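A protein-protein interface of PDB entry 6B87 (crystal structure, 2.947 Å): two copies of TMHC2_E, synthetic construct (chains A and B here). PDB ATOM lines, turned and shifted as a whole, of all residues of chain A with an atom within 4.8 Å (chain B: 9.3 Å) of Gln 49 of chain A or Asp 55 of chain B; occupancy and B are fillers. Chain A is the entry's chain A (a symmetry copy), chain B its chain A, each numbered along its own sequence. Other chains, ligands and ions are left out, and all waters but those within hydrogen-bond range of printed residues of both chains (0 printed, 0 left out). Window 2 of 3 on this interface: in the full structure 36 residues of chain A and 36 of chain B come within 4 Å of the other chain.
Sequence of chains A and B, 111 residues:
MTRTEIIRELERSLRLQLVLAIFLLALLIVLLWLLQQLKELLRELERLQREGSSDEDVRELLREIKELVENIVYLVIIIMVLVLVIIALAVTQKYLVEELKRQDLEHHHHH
CD2 of Leu 45 of chain B touches CD2 of Leu 45 of chain A, at 3.6 Å.
Leu 45 of chain A touches Leu 62 of chain B (CD2 to CD1, 3.96 Å).
Leu 62 of chain B touches Glu 46 of chain A.
Val 58 of chain B touches Gln 49 of chain A.
Val 58 of chain A touches Gln 49 of chain B.
Leu 48 of chain A touches none of the printed residues of chain B.
Gln 49 of chain A touches three residues of chain B.
Of the printed residues of chain B, Val 58 of chain A touches Gln 49.
Printed residues of chain A within 4 Å of Leu 45 of chain B: Leu 45.
Glu 46 of chain B touches none of the printed residues of chain A.
Of chain A, only Gln 49 (2.8 Å) comes within 4 Å of Asp 55 of chain B.
Of the printed residues of chain A, Val 58 of chain B touches Gln 49.
The nearest printed residue of chain A that does not touch Leu 45 of chain B is Val 58 of chain A (6.4 Å).
The side-chain amide oxygen (OE1) of Gln 49 of chain B lies close to the side-chain amide oxygen (OE1) of Gln 49 of chain A (3.0 Å).
OD1 of Asp 55 of chain B sits at hydrogen-bond distance from NE2 of Gln 49 of chain A (2.8 Å).
Leu 45 of chain B touches its own counterpart, Leu 45 of chain A.
Gln 49 of chain B touches its own counterpart, Gln 49 of chain A.
Gln 49 of chain A touches Val 58 of chain B, and with the chains exchanged Val 58 of chain A touches Gln 49 of chain B.
Positions printed for both chains: 45, 46, 48, 49, 50, 52 and 58.
Of the 7 pairs that touch across the chains among the printed residues, 4 have their exchanged pair printed and touching as well.
Printed residues of chain A that touch a printed residue of chain B: Leu 45, Glu 46, Gln 49 and Val 58.
Hydrophobic or aromatic side chains of chain A within 4 Å of the printed part of chain B: Leu 45 and Val 58.
Of the 17 printed residues of chain B, 5 touch a printed residue of chain A.
Hydrophobic or aromatic side chains of chain B that line the printed part of chain A: Leu 45, Val 58 and Leu 62.
Among the printed residues, 7 pairs touch across the chains.
Among the printed residues, no Asp or Glu carboxylate lies within 4 Å of a Lys or Arg side-chain nitrogen of the other chain.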
ATOM      1  N   LEU A  45     -12.905  -2.233 -12.340  1.00  0.00           N
ATOM      2  CA  LEU A  45     -13.914  -2.966 -13.089  1.00  0.00           C
ATOM      3  C   LEU A  45     -15.131  -3.218 -12.215  1.00  0.00           C
ATOM      4  O   LEU A  45     -16.265  -3.047 -12.668  1.00  0.00           O
ATOM      5  CB  LEU A  45     -13.318  -4.283 -13.596  1.00  0.00           C
ATOM      6  CG  LEU A  45     -14.174  -5.113 -14.545  1.00  0.00           C
ATOM      7  CD1 LEU A  45     -14.438  -4.312 -15.806  1.00  0.00           C
ATOM      8  CD2 LEU A  45     -13.441  -6.401 -14.878  1.00  0.00           C
ATOM      9  N   GLU A  46     -14.888  -3.576 -10.947  1.00  0.00           N
ATOM     10  CA  GLU A  46     -15.959  -3.691  -9.972  1.00  0.00           C
ATOM     11  C   GLU A  46     -16.702  -2.390  -9.828  1.00  0.00           C
ATOM     12  O   GLU A  46     -17.929  -2.385  -9.889  1.00  0.00           O
ATOM     13  CB  GLU A  46     -15.453  -4.086  -8.592  1.00  0.00           C
ATOM     14  CG  GLU A  46     -16.593  -4.181  -7.577  1.00  0.00           C
ATOM     15  CD  GLU A  46     -16.154  -4.383  -6.151  1.00  0.00           C
ATOM     16  OE1 GLU A  46     -14.976  -4.338  -5.898  1.00  0.00           O
ATOM     17  OE2 GLU A  46     -17.003  -4.597  -5.314  1.00  0.00           O
ATOM     18  N   ARG A  47     -15.962  -1.295  -9.632  1.00  0.00           N
ATOM     19  CA  ARG A  47     -16.571   0.016  -9.467  1.00  0.00           C
ATOM     20  C   ARG A  47     -17.446   0.415 -10.644  1.00  0.00           C
ATOM     21  O   ARG A  47     -18.533   0.943 -10.439  1.00  0.00           O
ATOM     22  CB  ARG A  47     -15.521   1.087  -9.240  1.00  0.00           C
ATOM     23  CG  ARG A  47     -16.108   2.487  -9.131  1.00  0.00           C
ATOM     24  CD  ARG A  47     -15.120   3.510  -8.691  1.00  0.00           C
ATOM     25  NE  ARG A  47     -14.012   3.691  -9.621  1.00  0.00           N
ATOM     26  CZ  ARG A  47     -14.044   4.440 -10.744  1.00  0.00           C
ATOM     27  NH1 ARG A  47     -15.137   5.079 -11.107  1.00  0.00           N
ATOM     28  NH2 ARG A  47     -12.954   4.543 -11.489  1.00  0.00           N
ATOM     29  N   LEU A  48     -17.007   0.140 -11.867  1.00  0.00           N
ATOM     30  CA  LEU A  48     -17.836   0.443 -13.026  1.00  0.00           C
ATOM     31  C   LEU A  48     -19.137  -0.338 -12.998  1.00  0.00           C
ATOM     32  O   LEU A  48     -20.200   0.190 -13.333  1.00  0.00           O
ATOM     33  CB  LEU A  48     -17.111   0.100 -14.327  1.00  0.00           C
ATOM     34  CG  LEU A  48     -15.905   0.960 -14.688  1.00  0.00           C
ATOM     35  CD1 LEU A  48     -15.314   0.437 -15.993  1.00  0.00           C
ATOM     36  CD2 LEU A  48     -16.331   2.410 -14.793  1.00  0.00           C
ATOM     37  N   GLN A  49     -19.061  -1.606 -12.592  1.00  0.00           N
ATOM     38  CA  GLN A  49     -20.251  -2.422 -12.533  1.00  0.00           C
ATOM     39  C   GLN A  49     -21.168  -1.961 -11.392  1.00  0.00           C
ATOM     40  O   GLN A  49     -22.390  -1.954 -11.546  1.00  0.00           O
ATOM     41  CB  GLN A  49     -19.880  -3.887 -12.376  1.00  0.00           C
ATOM     42  CG  GLN A  49     -21.036  -4.818 -12.679  1.00  0.00           C
ATOM     43  CD  GLN A  49     -21.451  -4.686 -14.142  1.00  0.00           C
ATOM     44  OE1 GLN A  49     -20.584  -4.603 -15.018  1.00  0.00           O
ATOM     45  NE2 GLN A  49     -22.752  -4.664 -14.413  1.00  0.00           N
ATOM     46  N   ARG A  50     -20.568  -1.534 -10.271  1.00  0.00           N
ATOM     47  CA  ARG A  50     -21.303  -0.970  -9.132  1.00  0.00           C
ATOM     48  C   ARG A  50     -22.054   0.289  -9.519  1.00  0.00           C
ATOM     49  O   ARG A  50     -23.219   0.468  -9.157  1.00  0.00           O
ATOM     50  CB  ARG A  50     -20.366  -0.599  -7.990  1.00  0.00           C
ATOM     51  CG  ARG A  50     -19.741  -1.731  -7.201  1.00  0.00           C
ATOM     52  CD  ARG A  50     -18.736  -1.188  -6.249  1.00  0.00           C
ATOM     53  NE  ARG A  50     -19.352  -0.311  -5.267  1.00  0.00           N
ATOM     54  CZ  ARG A  50     -19.833  -0.734  -4.084  1.00  0.00           C
ATOM     55  NH1 ARG A  50     -19.736  -2.006  -3.756  1.00  0.00           N
ATOM     56  NH2 ARG A  50     -20.397   0.128  -3.257  1.00  0.00           N
ATOM     57  N   GLU A  51     -21.377   1.157 -10.269  1.00  0.00           N
ATOM     58  CA  GLU A  51     -21.954   2.397 -10.762  1.00  0.00           C
ATOM     59  C   GLU A  51     -23.032   2.144 -11.805  1.00  0.00           C
ATOM     60  O   GLU A  51     -23.997   2.905 -11.899  1.00  0.00           O
ATOM     61  CB  GLU A  51     -20.855   3.291 -11.355  1.00  0.00           C
ATOM     62  CG  GLU A  51     -19.895   3.880 -10.324  1.00  0.00           C
ATOM     63  CD  GLU A  51     -18.734   4.624 -10.939  1.00  0.00           C
ATOM     64  OE1 GLU A  51     -18.699   4.758 -12.140  1.00  0.00           O
ATOM     65  OE2 GLU A  51     -17.880   5.061 -10.197  1.00  0.00           O
ATOM     66  N   GLY A  52     -22.877   1.077 -12.585  1.00  0.00           N
ATOM     67  CA  GLY A  52     -23.822   0.796 -13.644  1.00  0.00           C
ATOM     68  C   GLY A  52     -23.437   1.595 -14.872  1.00  0.00           C
ATOM     69  O   GLY A  52     -24.296   2.194 -15.525  1.00  0.00           O
ATOM     70  N   VAL A  58     -17.126  -0.530 -19.605  1.00  0.00           N
ATOM     71  CA  VAL A  58     -16.691  -1.797 -19.055  1.00  0.00           C
ATOM     72  C   VAL A  58     -15.863  -2.561 -20.064  1.00  0.00           C
ATOM     73  O   VAL A  58     -14.794  -3.057 -19.718  1.00  0.00           O
ATOM     74  CB  VAL A  58     -17.906  -2.644 -18.606  1.00  0.00           C
ATOM     75  CG1 VAL A  58     -17.463  -4.046 -18.222  1.00  0.00           C
ATOM     76  CG2 VAL A  58     -18.575  -1.974 -17.414  1.00  0.00           C
ATOM     77  N   LEU B  45     -16.557 -13.294 -18.554  1.00  0.00           N
ATOM     78  CA  LEU B  45     -16.918 -11.992 -18.013  1.00  0.00           C
ATOM     79  C   LEU B  45     -17.338 -11.060 -19.135  1.00  0.00           C
ATOM     80  O   LEU B  45     -18.334 -10.345 -19.007  1.00  0.00           O
ATOM     81  CB  LEU B  45     -15.729 -11.417 -17.235  1.00  0.00           C
ATOM     82  CG  LEU B  45     -15.970 -10.131 -16.452  1.00  0.00           C
ATOM     83  CD1 LEU B  45     -17.025 -10.384 -15.392  1.00  0.00           C
ATOM     84  CD2 LEU B  45     -14.666  -9.690 -15.810  1.00  0.00           C
ATOM     85  N   GLU B  46     -16.604 -11.108 -20.256  1.00  0.00           N
ATOM     86  CA  GLU B  46     -16.996 -10.385 -21.453  1.00  0.00           C
ATOM     87  C   GLU B  46     -18.362 -10.808 -21.918  1.00  0.00           C
ATOM     88  O   GLU B  46     -19.207  -9.953 -22.171  1.00  0.00           O
ATOM     89  CB  GLU B  46     -16.030 -10.601 -22.609  1.00  0.00           C
ATOM     90  CG  GLU B  46     -16.472  -9.849 -23.864  1.00  0.00           C
ATOM     91  CD  GLU B  46     -15.674 -10.160 -25.102  1.00  0.00           C
ATOM     92  OE1 GLU B  46     -14.849 -11.039 -25.051  1.00  0.00           O
ATOM     93  OE2 GLU B  46     -15.883  -9.507 -26.100  1.00  0.00           O
ATOM     94  N   LEU B  48     -20.845 -12.180 -20.302  1.00  0.00           N
ATOM     95  CA  LEU B  48     -21.908 -11.697 -19.431  1.00  0.00           C
ATOM     96  C   LEU B  48     -22.233 -10.239 -19.707  1.00  0.00           C
ATOM     97  O   LEU B  48     -23.400  -9.841 -19.710  1.00  0.00           O
ATOM     98  CB  LEU B  48     -21.513 -11.819 -17.960  1.00  0.00           C
ATOM     99  CG  LEU B  48     -21.392 -13.230 -17.397  1.00  0.00           C
ATOM    100  CD1 LEU B  48     -20.962 -13.131 -15.936  1.00  0.00           C
ATOM    101  CD2 LEU B  48     -22.713 -13.955 -17.557  1.00  0.00           C
ATOM    102  N   GLN B  49     -21.197  -9.434 -19.943  1.00  0.00           N
ATOM    103  CA  GLN B  49     -21.415  -8.033 -20.217  1.00  0.00           C
ATOM    104  C   GLN B  49     -22.062  -7.843 -21.594  1.00  0.00           C
ATOM    105  O   GLN B  49     -22.928  -6.983 -21.759  1.00  0.00           O
ATOM    106  CB  GLN B  49     -20.107  -7.265 -20.118  1.00  0.00           C
ATOM    107  CG  GLN B  49     -20.314  -5.768 -20.022  1.00  0.00           C
ATOM    108  CD  GLN B  49     -21.057  -5.419 -18.736  1.00  0.00           C
ATOM    109  OE1 GLN B  49     -20.755  -5.987 -17.681  1.00  0.00           O
ATOM    110  NE2 GLN B  49     -22.016  -4.501 -18.808  1.00  0.00           N
ATOM    111  N   ARG B  50     -21.670  -8.683 -22.566  1.00  0.00           N
ATOM    112  CA  ARG B  50     -22.267  -8.693 -23.906  1.00  0.00           C
ATOM    113  C   ARG B  50     -23.746  -9.026 -23.859  1.00  0.00           C
ATOM    114  O   ARG B  50     -24.561  -8.382 -24.522  1.00  0.00           O
ATOM    115  CB  ARG B  50     -21.604  -9.730 -24.805  1.00  0.00           C
ATOM    116  CG  ARG B  50     -20.197  -9.442 -25.286  1.00  0.00           C
ATOM    117  CD  ARG B  50     -19.656 -10.627 -26.002  1.00  0.00           C
ATOM    118  NE  ARG B  50     -20.431 -10.927 -27.196  1.00  0.00           N
ATOM    119  CZ  ARG B  50     -20.160 -10.417 -28.410  1.00  0.00           C
ATOM    120  NH1 ARG B  50     -19.127  -9.614 -28.566  1.00  0.00           N
ATOM    121  NH2 ARG B  50     -20.927 -10.725 -29.440  1.00  0.00           N
ATOM    122  N   GLY B  52     -25.626  -8.690 -21.204  1.00  0.00           N
ATOM    123  CA  GLY B  52     -26.335  -7.721 -20.397  1.00  0.00           C
ATOM    124  C   GLY B  52     -26.944  -8.428 -19.203  1.00  0.00           C
ATOM    125  O   GLY B  52     -28.104  -8.187 -18.857  1.00  0.00           O
ATOM    126  N   SER B  53     -26.158  -9.328 -18.599  1.00  0.00           N
ATOM    127  CA  SER B  53     -26.574 -10.086 -17.422  1.00  0.00           C
ATOM    128  C   SER B  53     -26.645  -9.170 -16.207  1.00  0.00           C
ATOM    129  O   SER B  53     -26.351  -7.974 -16.301  1.00  0.00           O
ATOM    130  CB  SER B  53     -25.609 -11.210 -17.131  1.00  0.00           C
ATOM    131  OG  SER B  53     -24.440 -10.702 -16.561  1.00  0.00           O
ATOM    132  N   SER B  54     -27.078  -9.712 -15.070  1.00  0.00           N
ATOM    133  CA  SER B  54     -27.292  -8.863 -13.910  1.00  0.00           C
ATOM    134  C   SER B  54     -26.001  -8.511 -13.215  1.00  0.00           C
ATOM    135  O   SER B  54     -24.967  -9.148 -13.433  1.00  0.00           O
ATOM    136  CB  SER B  54     -28.222  -9.533 -12.920  1.00  0.00           C
ATOM    137  OG  SER B  54     -27.625 -10.665 -12.358  1.00  0.00           O
ATOM    138  N   ASP B  55     -26.085  -7.527 -12.331  1.00  0.00           N
ATOM    139  CA  ASP B  55     -24.954  -7.115 -11.528  1.00  0.00           C
ATOM    140  C   ASP B  55     -24.516  -8.241 -10.610  1.00  0.00           C
ATOM    141  O   ASP B  55     -23.332  -8.371 -10.333  1.00  0.00           O
ATOM    142  CB  ASP B  55     -25.297  -5.871 -10.709  1.00  0.00           C
ATOM    143  CG  ASP B  55     -25.414  -4.606 -11.562  1.00  0.00           C
ATOM    144  OD1 ASP B  55     -24.949  -4.612 -12.678  1.00  0.00           O
ATOM    145  OD2 ASP B  55     -25.969  -3.645 -11.084  1.00  0.00           O
ATOM    146  N   GLU B  56     -25.468  -9.071 -10.166  1.00  0.00           N
ATOM    147  CA  GLU B  56     -25.161 -10.232  -9.340  1.00  0.00           C
ATOM    148  C   GLU B  56     -24.387 -11.293 -10.116  1.00  0.00           C
ATOM    149  O   GLU B  56     -23.444 -11.875  -9.582  1.00  0.00           O
ATOM    150  CB  GLU B  56     -26.443 -10.863  -8.798  1.00  0.00           C
ATOM    151  CG  GLU B  56     -27.205 -10.013  -7.796  1.00  0.00           C
ATOM    152  CD  GLU B  56     -28.448 -10.695  -7.286  1.00  0.00           C
ATOM    153  OE1 GLU B  56     -28.663 -11.835  -7.625  1.00  0.00           O
ATOM    154  OE2 GLU B  56     -29.184 -10.072  -6.556  1.00  0.00           O
ATOM    155  N   ASP B  57     -24.762 -11.512 -11.386  1.00  0.00           N
ATOM    156  CA  ASP B  57     -24.068 -12.487 -12.241  1.00  0.00           C
ATOM    157  C   ASP B  57     -22.615 -12.079 -12.479  1.00  0.00           C
ATOM    158  O   ASP B  57     -21.696 -12.894 -12.343  1.00  0.00           O
ATOM    159  CB  ASP B  57     -24.761 -12.591 -13.613  1.00  0.00           C
ATOM    160  CG  ASP B  57     -26.134 -13.244 -13.592  1.00  0.00           C
ATOM    161  OD1 ASP B  57     -26.275 -14.289 -13.003  1.00  0.00           O
ATOM    162  OD2 ASP B  57     -27.052 -12.655 -14.135  1.00  0.00           O
ATOM    163  N   VAL B  58     -22.427 -10.803 -12.823  1.00  0.00           N
ATOM    164  CA  VAL B  58     -21.114 -10.262 -13.107  1.00  0.00           C
ATOM    165  C   VAL B  58     -20.283 -10.188 -11.846  1.00  0.00           C
ATOM    166  O   VAL B  58     -19.131 -10.615 -11.854  1.00  0.00           O
ATOM    167  CB  VAL B  58     -21.228  -8.863 -13.759  1.00  0.00           C
ATOM    168  CG1 VAL B  58     -19.858  -8.215 -13.867  1.00  0.00           C
ATOM    169  CG2 VAL B  58     -21.841  -9.001 -15.145  1.00  0.00           C
ATOM    170  N   ARG B  59     -20.865  -9.656 -10.771  1.00  0.00           N
ATOM    171  CA  ARG B  59     -20.202  -9.547  -9.480  1.00  0.00           C
ATOM    172  C   ARG B  59     -19.716 -10.886  -8.964  1.00  0.00           C
ATOM    173  O   ARG B  59     -18.592 -10.978  -8.481  1.00  0.00           O
ATOM    174  CB  ARG B  59     -21.123  -8.938  -8.460  1.00  0.00           C
ATOM    175  CG  ARG B  59     -20.536  -8.727  -7.089  1.00  0.00           C
ATOM    176  CD  ARG B  59     -21.621  -8.462  -6.126  1.00  0.00           C
ATOM    177  NE  ARG B  59     -22.448  -9.642  -5.963  1.00  0.00           N
ATOM    178  CZ  ARG B  59     -23.690  -9.655  -5.452  1.00  0.00           C
ATOM    179  NH1 ARG B  59     -24.253  -8.538  -5.043  1.00  0.00           N
ATOM    180  NH2 ARG B  59     -24.339 -10.802  -5.365  1.00  0.00           N
ATOM    181  N   GLU B  60     -20.558 -11.921  -9.059  1.00  0.00           N
ATOM    182  CA  GLU B  60     -20.173 -13.276  -8.672  1.00  0.00           C
ATOM    183  C   GLU B  60     -18.915 -13.731  -9.390  1.00  0.00           C
ATOM    184  O   GLU B  60     -17.959 -14.180  -8.753  1.00  0.00           O
ATOM    185  CB  GLU B  60     -21.309 -14.259  -8.987  1.00  0.00           C
ATOM    186  CG  GLU B  60     -20.986 -15.724  -8.723  1.00  0.00           C
ATOM    187  CD  GLU B  60     -22.113 -16.641  -9.119  1.00  0.00           C
ATOM    188  OE1 GLU B  60     -23.191 -16.154  -9.354  1.00  0.00           O
ATOM    189  OE2 GLU B  60     -21.895 -17.827  -9.196  1.00  0.00           O
ATOM    190  N   LEU B  61     -18.920 -13.600 -10.717  1.00  0.00           N
ATOM    191  CA  LEU B  61     -17.781 -13.996 -11.524  1.00  0.00           C
ATOM    192  C   LEU B  61     -16.548 -13.157 -11.225  1.00  0.00           C
ATOM    193  O   LEU B  61     -15.443 -13.690 -11.138  1.00  0.00           O
ATOM    194  CB  LEU B  61     -18.135 -13.909 -13.003  1.00  0.00           C
ATOM    195  CG  LEU B  61     -17.013 -14.302 -13.957  1.00  0.00           C
ATOM    196  CD1 LEU B  61     -16.537 -15.696 -13.629  1.00  0.00           C
ATOM    197  CD2 LEU B  61     -17.535 -14.273 -15.371  1.00  0.00           C
ATOM    198  N   LEU B  62     -16.735 -11.854 -11.062  1.00  0.00           N
ATOM    199  CA  LEU B  62     -15.646 -10.948 -10.745  1.00  0.00           C
ATOM    200  C   LEU B  62     -15.040 -11.231  -9.359  1.00  0.00           C
ATOM    201  O   LEU B  62     -13.829 -11.120  -9.180  1.00  0.00           O
ATOM    202  CB  LEU B  62     -16.138  -9.512 -10.859  1.00  0.00           C
ATOM    203  CG  LEU B  62     -15.068  -8.439 -10.691  1.00  0.00           C
ATOM    204  CD1 LEU B  62     -13.947  -8.692 -11.691  1.00  0.00           C
ATOM    205  CD2 LEU B  62     -15.703  -7.079 -10.938  1.00  0.00           C
ATOM    206  N   ARG B  63     -15.862 -11.629  -8.394  1.00  0.00           N
ATOM    207  CA  ARG B  63     -15.349 -12.064  -7.099  1.00  0.00           C
ATOM    208  C   ARG B  63     -14.466 -13.316  -7.230  1.00  0.00           C
ATOM    209  O   ARG B  63     -13.434 -13.416  -6.560  1.00  0.00           O
ATOM    210  CB  ARG B  63     -16.499 -12.347  -6.136  1.00  0.00           C
ATOM    211  CG  ARG B  63     -17.229 -11.122  -5.585  1.00  0.00           C
ATOM    212  CD  ARG B  63     -18.433 -11.516  -4.799  1.00  0.00           C
ATOM    213  NE  ARG B  63     -19.057 -10.385  -4.123  1.00  0.00           N
ATOM    214  CZ  ARG B  63     -20.185 -10.464  -3.387  1.00  0.00           C
ATOM    215  NH1 ARG B  63     -20.806 -11.617  -3.261  1.00  0.00           N
ATOM    216  NH2 ARG B  63     -20.666  -9.387  -2.788  1.00  0.00           N
